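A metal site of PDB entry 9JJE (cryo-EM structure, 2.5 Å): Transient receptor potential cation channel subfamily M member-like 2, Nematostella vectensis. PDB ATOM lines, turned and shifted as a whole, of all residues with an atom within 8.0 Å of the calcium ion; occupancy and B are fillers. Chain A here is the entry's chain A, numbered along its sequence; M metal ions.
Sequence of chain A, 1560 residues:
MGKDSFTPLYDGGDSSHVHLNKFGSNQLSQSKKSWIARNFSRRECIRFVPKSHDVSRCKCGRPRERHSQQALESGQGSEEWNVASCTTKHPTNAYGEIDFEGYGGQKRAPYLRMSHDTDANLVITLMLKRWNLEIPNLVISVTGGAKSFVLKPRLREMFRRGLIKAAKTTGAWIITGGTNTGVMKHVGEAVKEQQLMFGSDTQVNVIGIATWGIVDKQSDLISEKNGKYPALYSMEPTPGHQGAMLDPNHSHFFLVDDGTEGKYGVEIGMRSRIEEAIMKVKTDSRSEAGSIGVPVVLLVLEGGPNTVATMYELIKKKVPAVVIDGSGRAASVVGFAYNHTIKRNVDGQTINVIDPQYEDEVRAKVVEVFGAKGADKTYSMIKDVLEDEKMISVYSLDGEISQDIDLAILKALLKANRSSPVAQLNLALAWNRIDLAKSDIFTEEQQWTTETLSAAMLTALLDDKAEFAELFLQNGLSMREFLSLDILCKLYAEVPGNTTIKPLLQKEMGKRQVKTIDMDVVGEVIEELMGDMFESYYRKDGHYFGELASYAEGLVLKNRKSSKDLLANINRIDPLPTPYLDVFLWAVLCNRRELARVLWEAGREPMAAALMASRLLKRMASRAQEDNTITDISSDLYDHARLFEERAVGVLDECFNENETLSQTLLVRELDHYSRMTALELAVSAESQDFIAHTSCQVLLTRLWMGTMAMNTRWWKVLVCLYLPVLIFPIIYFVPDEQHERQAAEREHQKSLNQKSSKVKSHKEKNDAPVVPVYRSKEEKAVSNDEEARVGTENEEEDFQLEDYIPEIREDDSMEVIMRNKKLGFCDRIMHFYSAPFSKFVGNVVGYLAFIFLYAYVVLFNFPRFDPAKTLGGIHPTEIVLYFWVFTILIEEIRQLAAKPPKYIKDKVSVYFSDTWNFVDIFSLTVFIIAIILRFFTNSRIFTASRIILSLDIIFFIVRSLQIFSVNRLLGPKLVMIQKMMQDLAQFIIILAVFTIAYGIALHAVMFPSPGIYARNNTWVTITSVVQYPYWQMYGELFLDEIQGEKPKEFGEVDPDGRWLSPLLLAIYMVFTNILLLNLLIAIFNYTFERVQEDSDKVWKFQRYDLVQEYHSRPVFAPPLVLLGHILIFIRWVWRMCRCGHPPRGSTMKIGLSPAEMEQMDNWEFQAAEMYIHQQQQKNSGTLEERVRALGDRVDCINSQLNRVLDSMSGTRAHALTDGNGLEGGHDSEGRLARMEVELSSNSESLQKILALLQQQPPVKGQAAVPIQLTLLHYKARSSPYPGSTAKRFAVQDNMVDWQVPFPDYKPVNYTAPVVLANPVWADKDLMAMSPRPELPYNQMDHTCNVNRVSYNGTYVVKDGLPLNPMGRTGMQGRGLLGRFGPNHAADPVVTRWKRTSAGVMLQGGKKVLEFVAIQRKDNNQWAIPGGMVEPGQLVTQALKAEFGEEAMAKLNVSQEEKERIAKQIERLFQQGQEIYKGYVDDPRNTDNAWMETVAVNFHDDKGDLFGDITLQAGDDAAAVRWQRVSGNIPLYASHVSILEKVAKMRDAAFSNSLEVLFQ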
ATOM      1  N   ILE A 889     -34.036  29.607  -0.413  1.00  0.00           N
ATOM      2  CA  ILE A 889     -33.006  28.734   0.154  1.00  0.00           C
ATOM      3  C   ILE A 889     -31.622  29.083  -0.411  1.00  0.00           C
ATOM      4  O   ILE A 889     -30.610  29.026   0.290  1.00  0.00           O
ATOM      5  CB  ILE A 889     -33.385  27.254  -0.077  1.00  0.00           C
ATOM      6  CG1 ILE A 889     -34.677  26.913   0.657  1.00  0.00           C
ATOM      7  CG2 ILE A 889     -32.304  26.301   0.421  1.00  0.00           C
ATOM      8  CD1 ILE A 889     -35.242  25.561   0.307  1.00  0.00           C
ATOM      9  N   GLU A 892     -30.544  32.172   1.248  1.00  0.00           N
ATOM     10  CA  GLU A 892     -30.203  31.738   2.592  1.00  0.00           C
ATOM     11  C   GLU A 892     -28.788  31.163   2.671  1.00  0.00           C
ATOM     12  O   GLU A 892     -28.026  31.505   3.578  1.00  0.00           O
ATOM     13  CB  GLU A 892     -31.218  30.695   3.062  1.00  0.00           C
ATOM     14  CG  GLU A 892     -30.861  29.962   4.343  1.00  0.00           C
ATOM     15  CD  GLU A 892     -30.827  30.858   5.562  1.00  0.00           C
ATOM     16  OE1 GLU A 892     -31.600  31.831   5.610  1.00  0.00           O
ATOM     17  OE2 GLU A 892     -29.996  30.589   6.444  1.00  0.00           O
ATOM     18  N   GLU A 893     -28.420  30.318   1.705  1.00  0.00           N
ATOM     19  CA  GLU A 893     -27.076  29.744   1.735  1.00  0.00           C
ATOM     20  C   GLU A 893     -26.010  30.758   1.333  1.00  0.00           C
ATOM     21  O   GLU A 893     -24.882  30.694   1.831  1.00  0.00           O
ATOM     22  CB  GLU A 893     -27.024  28.506   0.833  1.00  0.00           C
ATOM     23  CG  GLU A 893     -27.916  27.372   1.310  1.00  0.00           C
ATOM     24  CD  GLU A 893     -27.487  26.799   2.657  1.00  0.00           C
ATOM     25  OE1 GLU A 893     -26.272  26.737   2.934  1.00  0.00           O
ATOM     26  OE2 GLU A 893     -28.377  26.416   3.440  1.00  0.00           O
ATOM     27  N   ILE A 894     -26.350  31.732   0.474  1.00  0.00           N
ATOM     28  CA  ILE A 894     -25.440  32.823   0.178  1.00  0.00           C
ATOM     29  C   ILE A 894     -25.240  33.699   1.408  1.00  0.00           C
ATOM     30  O   ILE A 894     -24.124  34.169   1.685  1.00  0.00           O
ATOM     31  CB  ILE A 894     -25.939  33.623  -1.042  1.00  0.00           C
ATOM     32  CG1 ILE A 894     -25.845  32.774  -2.309  1.00  0.00           C
ATOM     33  CG2 ILE A 894     -25.178  34.926  -1.251  1.00  0.00           C
ATOM     34  CD1 ILE A 894     -26.567  33.362  -3.492  1.00  0.00           C
ATOM     35  N   ARG A 895     -26.306  33.904   2.197  1.00  0.00           N
ATOM     36  CA  ARG A 895     -26.209  34.633   3.455  1.00  0.00           C
ATOM     37  C   ARG A 895     -25.334  33.887   4.450  1.00  0.00           C
ATOM     38  O   ARG A 895     -24.543  34.499   5.173  1.00  0.00           O
ATOM     39  CB  ARG A 895     -27.613  34.877   4.027  1.00  0.00           C
ATOM     40  CG  ARG A 895     -27.755  35.913   5.155  1.00  0.00           C
ATOM     41  CD  ARG A 895     -27.585  35.326   6.549  1.00  0.00           C
ATOM     42  NE  ARG A 895     -28.460  34.182   6.782  1.00  0.00           N
ATOM     43  CZ  ARG A 895     -28.232  33.266   7.720  1.00  0.00           C
ATOM     44  NH1 ARG A 895     -27.157  33.354   8.497  1.00  0.00           N
ATOM     45  NH2 ARG A 895     -29.066  32.251   7.898  1.00  0.00           N
ATOM     46  N   GLN A 896     -25.481  32.563   4.520  1.00  0.00           N
ATOM     47  CA  GLN A 896     -24.669  31.764   5.435  1.00  0.00           C
ATOM     48  C   GLN A 896     -23.210  31.720   4.994  1.00  0.00           C
ATOM     49  O   GLN A 896     -22.321  31.627   5.850  1.00  0.00           O
ATOM     50  CB  GLN A 896     -25.223  30.341   5.548  1.00  0.00           C
ATOM     51  CG  GLN A 896     -26.569  30.242   6.260  1.00  0.00           C
ATOM     52  CD  GLN A 896     -27.065  28.817   6.346  1.00  0.00           C
ATOM     53  OE1 GLN A 896     -26.423  27.898   5.834  1.00  0.00           O
ATOM     54  NE2 GLN A 896     -28.199  28.610   7.006  1.00  0.00           N
ATOM     55  N   LEU A 897     -22.951  31.792   3.687  1.00  0.00           N
ATOM     56  CA  LEU A 897     -21.578  31.920   3.211  1.00  0.00           C
ATOM     57  C   LEU A 897     -20.997  33.283   3.572  1.00  0.00           C
ATOM     58  O   LEU A 897     -19.837  33.379   3.992  1.00  0.00           O
ATOM     59  CB  LEU A 897     -21.530  31.684   1.705  1.00  0.00           C
ATOM     60  CG  LEU A 897     -20.176  31.815   1.006  1.00  0.00           C
ATOM     61  CD1 LEU A 897     -19.170  30.813   1.542  1.00  0.00           C
ATOM     62  CD2 LEU A 897     -20.329  31.647  -0.497  1.00  0.00           C
ATOM     63  N   LYS A 900     -19.878  34.163   7.447  1.00  0.00           N
ATOM     64  CA  LYS A 900     -18.849  33.387   8.119  1.00  0.00           C
ATOM     65  C   LYS A 900     -17.832  34.316   8.781  1.00  0.00           C
ATOM     66  O   LYS A 900     -17.569  35.415   8.280  1.00  0.00           O
ATOM     67  CB  LYS A 900     -18.171  32.444   7.130  1.00  0.00           C
ATOM     68  CG  LYS A 900     -19.101  31.343   6.626  1.00  0.00           C
ATOM     69  CD  LYS A 900     -19.546  30.456   7.780  1.00  0.00           C
ATOM     70  CE  LYS A 900     -20.449  29.327   7.325  1.00  0.00           C
ATOM     71  NZ  LYS A 900     -20.937  28.505   8.472  1.00  0.00           N
ATOM     72  N   TYR A 912     -17.409  27.385   5.382  1.00  0.00           N
ATOM     73  CA  TYR A 912     -18.760  27.011   4.953  1.00  0.00           C
ATOM     74  C   TYR A 912     -18.865  25.529   4.642  1.00  0.00           C
ATOM     75  O   TYR A 912     -19.838  24.879   5.043  1.00  0.00           O
ATOM     76  CB  TYR A 912     -19.142  27.855   3.730  1.00  0.00           C
ATOM     77  CG  TYR A 912     -20.523  27.572   3.180  1.00  0.00           C
ATOM     78  CD1 TYR A 912     -21.651  28.074   3.818  1.00  0.00           C
ATOM     79  CD2 TYR A 912     -20.682  26.837   2.017  1.00  0.00           C
ATOM     80  CE1 TYR A 912     -22.919  27.825   3.306  1.00  0.00           C
ATOM     81  CE2 TYR A 912     -21.938  26.583   1.511  1.00  0.00           C
ATOM     82  CZ  TYR A 912     -23.054  27.080   2.153  1.00  0.00           C
ATOM     83  OH  TYR A 912     -24.291  26.819   1.635  1.00  0.00           O
ATOM     84  N   ASP A 915     -19.042  21.610   7.350  1.00  0.00           N
ATOM     85  CA  ASP A 915     -20.107  20.676   7.686  1.00  0.00           C
ATOM     86  C   ASP A 915     -20.696  20.060   6.415  1.00  0.00           C
ATOM     87  O   ASP A 915     -20.707  20.689   5.346  1.00  0.00           O
ATOM     88  CB  ASP A 915     -21.204  21.348   8.527  1.00  0.00           C
ATOM     89  CG  ASP A 915     -21.757  22.621   7.905  1.00  0.00           C
ATOM     90  OD1 ASP A 915     -21.226  23.073   6.864  1.00  0.00           O
ATOM     91  OD2 ASP A 915     -22.724  23.178   8.456  1.00  0.00           O
ATOM     92  N   THR A 916     -21.180  18.820   6.543  1.00  0.00           N
ATOM     93  CA  THR A 916     -21.730  18.087   5.405  1.00  0.00           C
ATOM     94  C   THR A 916     -23.100  18.623   4.981  1.00  0.00           C
ATOM     95  O   THR A 916     -23.515  18.422   3.828  1.00  0.00           O
ATOM     96  CB  THR A 916     -21.796  16.596   5.760  1.00  0.00           C
ATOM     97  OG1 THR A 916     -20.561  16.207   6.372  1.00  0.00           O
ATOM     98  CG2 THR A 916     -21.977  15.708   4.531  1.00  0.00           C
ATOM     99  N   TRP A 917     -23.778  19.341   5.879  1.00  0.00           N
ATOM    100  CA  TRP A 917     -25.091  19.895   5.561  1.00  0.00           C
ATOM    101  C   TRP A 917     -24.999  20.984   4.501  1.00  0.00           C
ATOM    102  O   TRP A 917     -25.911  21.127   3.676  1.00  0.00           O
ATOM    103  CB  TRP A 917     -25.741  20.457   6.829  1.00  0.00           C
ATOM    104  CG  TRP A 917     -25.943  19.403   7.871  1.00  0.00           C
ATOM    105  CD1 TRP A 917     -25.183  19.191   8.977  1.00  0.00           C
ATOM    106  CD2 TRP A 917     -26.939  18.376   7.869  1.00  0.00           C
ATOM    107  NE1 TRP A 917     -25.663  18.115   9.687  1.00  0.00           N
ATOM    108  CE2 TRP A 917     -26.746  17.601   9.025  1.00  0.00           C
ATOM    109  CE3 TRP A 917     -27.995  18.051   7.002  1.00  0.00           C
ATOM    110  CZ2 TRP A 917     -27.558  16.510   9.339  1.00  0.00           C
ATOM    111  CZ3 TRP A 917     -28.798  16.983   7.317  1.00  0.00           C
ATOM    112  CH2 TRP A 917     -28.577  16.219   8.477  1.00  0.00           C
ATOM    113  N   ASN A 918     -23.888  21.712   4.459  1.00  0.00           N
ATOM    114  CA  ASN A 918     -23.692  22.675   3.376  1.00  0.00           C
ATOM    115  C   ASN A 918     -23.363  21.981   2.062  1.00  0.00           C
ATOM    116  O   ASN A 918     -23.708  22.495   1.002  1.00  0.00           O
ATOM    117  CB  ASN A 918     -22.598  23.676   3.748  1.00  0.00           C
ATOM    118  CG  ASN A 918     -23.044  24.671   4.800  1.00  0.00           C
ATOM    119  OD1 ASN A 918     -24.183  25.150   4.770  1.00  0.00           O
ATOM    120  ND2 ASN A 918     -22.163  25.001   5.726  1.00  0.00           N
ATOM    121  N   PHE A 919     -22.720  20.800   2.108  1.00  0.00           N
ATOM    122  CA  PHE A 919     -22.558  20.009   0.893  1.00  0.00           C
ATOM    123  C   PHE A 919     -23.903  19.545   0.354  1.00  0.00           C
ATOM    124  O   PHE A 919     -24.148  19.605  -0.858  1.00  0.00           O
ATOM    125  CB  PHE A 919     -21.660  18.798   1.150  1.00  0.00           C
ATOM    126  CG  PHE A 919     -20.201  19.137   1.325  1.00  0.00           C
ATOM    127  CD1 PHE A 919     -19.398  19.373   0.211  1.00  0.00           C
ATOM    128  CD2 PHE A 919     -19.631  19.183   2.586  1.00  0.00           C
ATOM    129  CE1 PHE A 919     -18.063  19.677   0.356  1.00  0.00           C
ATOM    130  CE2 PHE A 919     -18.284  19.482   2.735  1.00  0.00           C
ATOM    131  CZ  PHE A 919     -17.500  19.730   1.620  1.00  0.00           C
ATOM    132  N   VAL A 920     -24.803  19.109   1.254  1.00  0.00           N
ATOM    133  CA  VAL A 920     -26.142  18.690   0.851  1.00  0.00           C
ATOM    134  C   VAL A 920     -26.934  19.882   0.301  1.00  0.00           C
ATOM    135  O   VAL A 920     -27.638  19.760  -0.715  1.00  0.00           O
ATOM    136  CB  VAL A 920     -26.865  18.020   2.032  1.00  0.00           C
ATOM    137  CG1 VAL A 920     -28.296  17.642   1.660  1.00  0.00           C
ATOM    138  CG2 VAL A 920     -26.091  16.785   2.479  1.00  0.00           C
ATOM    139  N   ASP A 921     -26.769  21.055   0.929  1.00  0.00           N
ATOM    140  CA  ASP A 921     -27.426  22.281   0.463  1.00  0.00           C
ATOM    141  C   ASP A 921     -26.961  22.693  -0.932  1.00  0.00           C
ATOM    142  O   ASP A 921     -27.781  22.928  -1.815  1.00  0.00           O
ATOM    143  CB  ASP A 921     -27.179  23.411   1.461  1.00  0.00           C
ATOM    144  CG  ASP A 921     -28.110  23.360   2.640  1.00  0.00           C
ATOM    145  OD1 ASP A 921     -29.290  23.026   2.443  1.00  0.00           O
ATOM    146  OD2 ASP A 921     -27.657  23.626   3.766  1.00  0.00           O
ATOM    147  N   ILE A 922     -25.640  22.780  -1.129  1.00  0.00           N
ATOM    148  CA  ILE A 922     -25.102  23.213  -2.418  1.00  0.00           C
ATOM    149  C   ILE A 922     -25.411  22.201  -3.508  1.00  0.00           C
ATOM    150  O   ILE A 922     -25.757  22.586  -4.641  1.00  0.00           O
ATOM    151  CB  ILE A 922     -23.591  23.510  -2.296  1.00  0.00           C
ATOM    152  CG1 ILE A 922     -23.351  24.690  -1.352  1.00  0.00           C
ATOM    153  CG2 ILE A 922     -22.947  23.793  -3.642  1.00  0.00           C
ATOM    154  CD1 ILE A 922     -24.027  25.975  -1.791  1.00  0.00           C
ATOM    155  N   LEU A 925     -29.298  22.559  -4.266  1.00  0.00           N
ATOM    156  CA  LEU A 925     -29.579  23.801  -4.972  1.00  0.00           C
ATOM    157  C   LEU A 925     -29.035  23.783  -6.398  1.00  0.00           C
ATOM    158  O   LEU A 925     -29.716  24.239  -7.324  1.00  0.00           O
ATOM    159  CB  LEU A 925     -29.002  24.985  -4.202  1.00  0.00           C
ATOM    160  CG  LEU A 925     -29.659  25.373  -2.870  1.00  0.00           C
ATOM    161  CD1 LEU A 925     -28.805  26.400  -2.163  1.00  0.00           C
ATOM    162  CD2 LEU A 925     -31.051  25.906  -3.093  1.00  0.00           C
ATOM    163  N   ARG A 960     -31.448  16.867   3.469  1.00  0.00           N
ATOM    164  CA  ARG A 960     -31.257  18.107   4.225  1.00  0.00           C
ATOM    165  C   ARG A 960     -32.272  18.247   5.362  1.00  0.00           C
ATOM    166  O   ARG A 960     -31.957  18.859   6.392  1.00  0.00           O
ATOM    167  CB  ARG A 960     -31.311  19.300   3.260  1.00  0.00           C
ATOM    168  CG  ARG A 960     -31.010  20.629   3.909  1.00  0.00           C
ATOM    169  CD  ARG A 960     -29.631  20.563   4.554  1.00  0.00           C
ATOM    170  NE  ARG A 960     -29.250  21.821   5.175  1.00  0.00           N
ATOM    171  CZ  ARG A 960     -29.526  22.144   6.439  1.00  0.00           C
ATOM    172  NH1 ARG A 960     -30.181  21.295   7.213  1.00  0.00           N
ATOM    173  NH2 ARG A 960     -29.128  23.309   6.918  1.00  0.00           N
ATOM    174  N   GLN A 963     -31.585  17.127   9.430  1.00  0.00           N
ATOM    175  CA  GLN A 963     -31.008  17.868  10.548  1.00  0.00           C
ATOM    176  C   GLN A 963     -32.052  18.274  11.578  1.00  0.00           C
ATOM    177  O   GLN A 963     -31.704  18.503  12.748  1.00  0.00           O
ATOM    178  CB  GLN A 963     -30.238  19.096  10.026  1.00  0.00           C
ATOM    179  CG  GLN A 963     -29.335  19.799  11.060  1.00  0.00           C
ATOM    180  CD  GLN A 963     -28.590  20.990  10.501  1.00  0.00           C
ATOM    181  OE1 GLN A 963     -28.745  21.340   9.341  1.00  0.00           O
ATOM    182  NE2 GLN A 963     -27.773  21.626  11.348  1.00  0.00           N
ATOM    183  N   GLU A1110     -26.774  26.505  13.806  1.00  0.00           N
ATOM    184  CA  GLU A1110     -27.508  26.560  12.553  1.00  0.00           C
ATOM    185  C   GLU A1110     -28.666  27.543  12.621  1.00  0.00           C
ATOM    186  O   GLU A1110     -28.952  28.230  11.633  1.00  0.00           O
ATOM    187  CB  GLU A1110     -28.008  25.158  12.192  1.00  0.00           C
ATOM    188  CG  GLU A1110     -28.826  25.047  10.895  1.00  0.00           C
ATOM    189  CD  GLU A1110     -28.011  25.320   9.642  1.00  0.00           C
ATOM    190  OE1 GLU A1110     -26.785  25.072   9.651  1.00  0.00           O
ATOM    191  OE2 GLU A1110     -28.587  25.782   8.642  1.00  0.00           O
ATOM    192  N   ARG A1114     -30.000  32.708  11.658  1.00  0.00           N
ATOM    193  CA  ARG A1114     -31.099  32.843  10.718  1.00  0.00           C
ATOM    194  C   ARG A1114     -31.734  34.235  10.834  1.00  0.00           C
ATOM    195  O   ARG A1114     -31.567  34.913  11.855  1.00  0.00           O
ATOM    196  CB  ARG A1114     -32.132  31.753  10.976  1.00  0.00           C
ATOM    197  CG  ARG A1114     -31.628  30.333  10.833  1.00  0.00           C
ATOM    198  CD  ARG A1114     -31.284  30.015   9.396  1.00  0.00           C
ATOM    199  NE  ARG A1114     -30.892  28.611   9.205  1.00  0.00           N
ATOM    200  CZ  ARG A1114     -31.739  27.637   8.914  1.00  0.00           C
ATOM    201  NH1 ARG A1114     -33.037  27.899   8.792  1.00  0.00           N
ATOM    202  NH2 ARG A1114     -31.305  26.399   8.747  1.00  0.00           N
HETATM  203 CA    CA M   1     -26.705  25.481   5.178  1.00  0.00          CA
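The side-chain carboxylate of Asp 921 lies within salt-bridge range of the guanidinium group of Arg 960 (3.0 Å).
NE2 of Gln 896 lies close to NE of Arg 1114, at 3.5 Å.
The side-chain amide nitrogen of Gln 896 sits at hydrogen-bond distance from the side-chain carboxylate of Glu 892 (2.7 Å).
ND2 of Asn 918 sits at hydrogen-bond distance from O of Tyr 912, 2.4 Å away.
The side-chain carboxylate of Asp 915 lies within hydrogen-bond range of the side-chain amide nitrogen of Asn 918 (2.4 Å).
NH2 of Arg 960 lies within salt-bridge range of OE2 of Glu 1110 (3.1 Å).
OE1 of Gln 963 is in hydrogen-bond range of NH1 of Arg 960.
The side-chain carboxylate (OE2) of Glu 1110 lies within salt-bridge range of the guanidinium group (NH2) of Arg 1114 (2.8 Å).
Merely in contact with the calcium ion: Arg 960 (3.7 Å) and Glu 1110 (3.95 Å).
Within 4 Å of the calcium ion: Glu 893, Gln 896, Asn 918, Asp 921, Arg 960 and Glu 1110.
OD2 of Asp 921 binds the calcium ion, 2.5 Å away.
OE1 of Gln 896 binds the calcium ion (2.5 Å).
The side-chain amide oxygen (OD1) of Asn 918 is bound to the calcium ion, at 2.6 Å.
The side-chain carboxylate (OE2) of Glu 893 binds the calcium ion, at 2.6 Å.
The calcium ion is bound by OE1 of Glu 893, at 2.6 Å.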
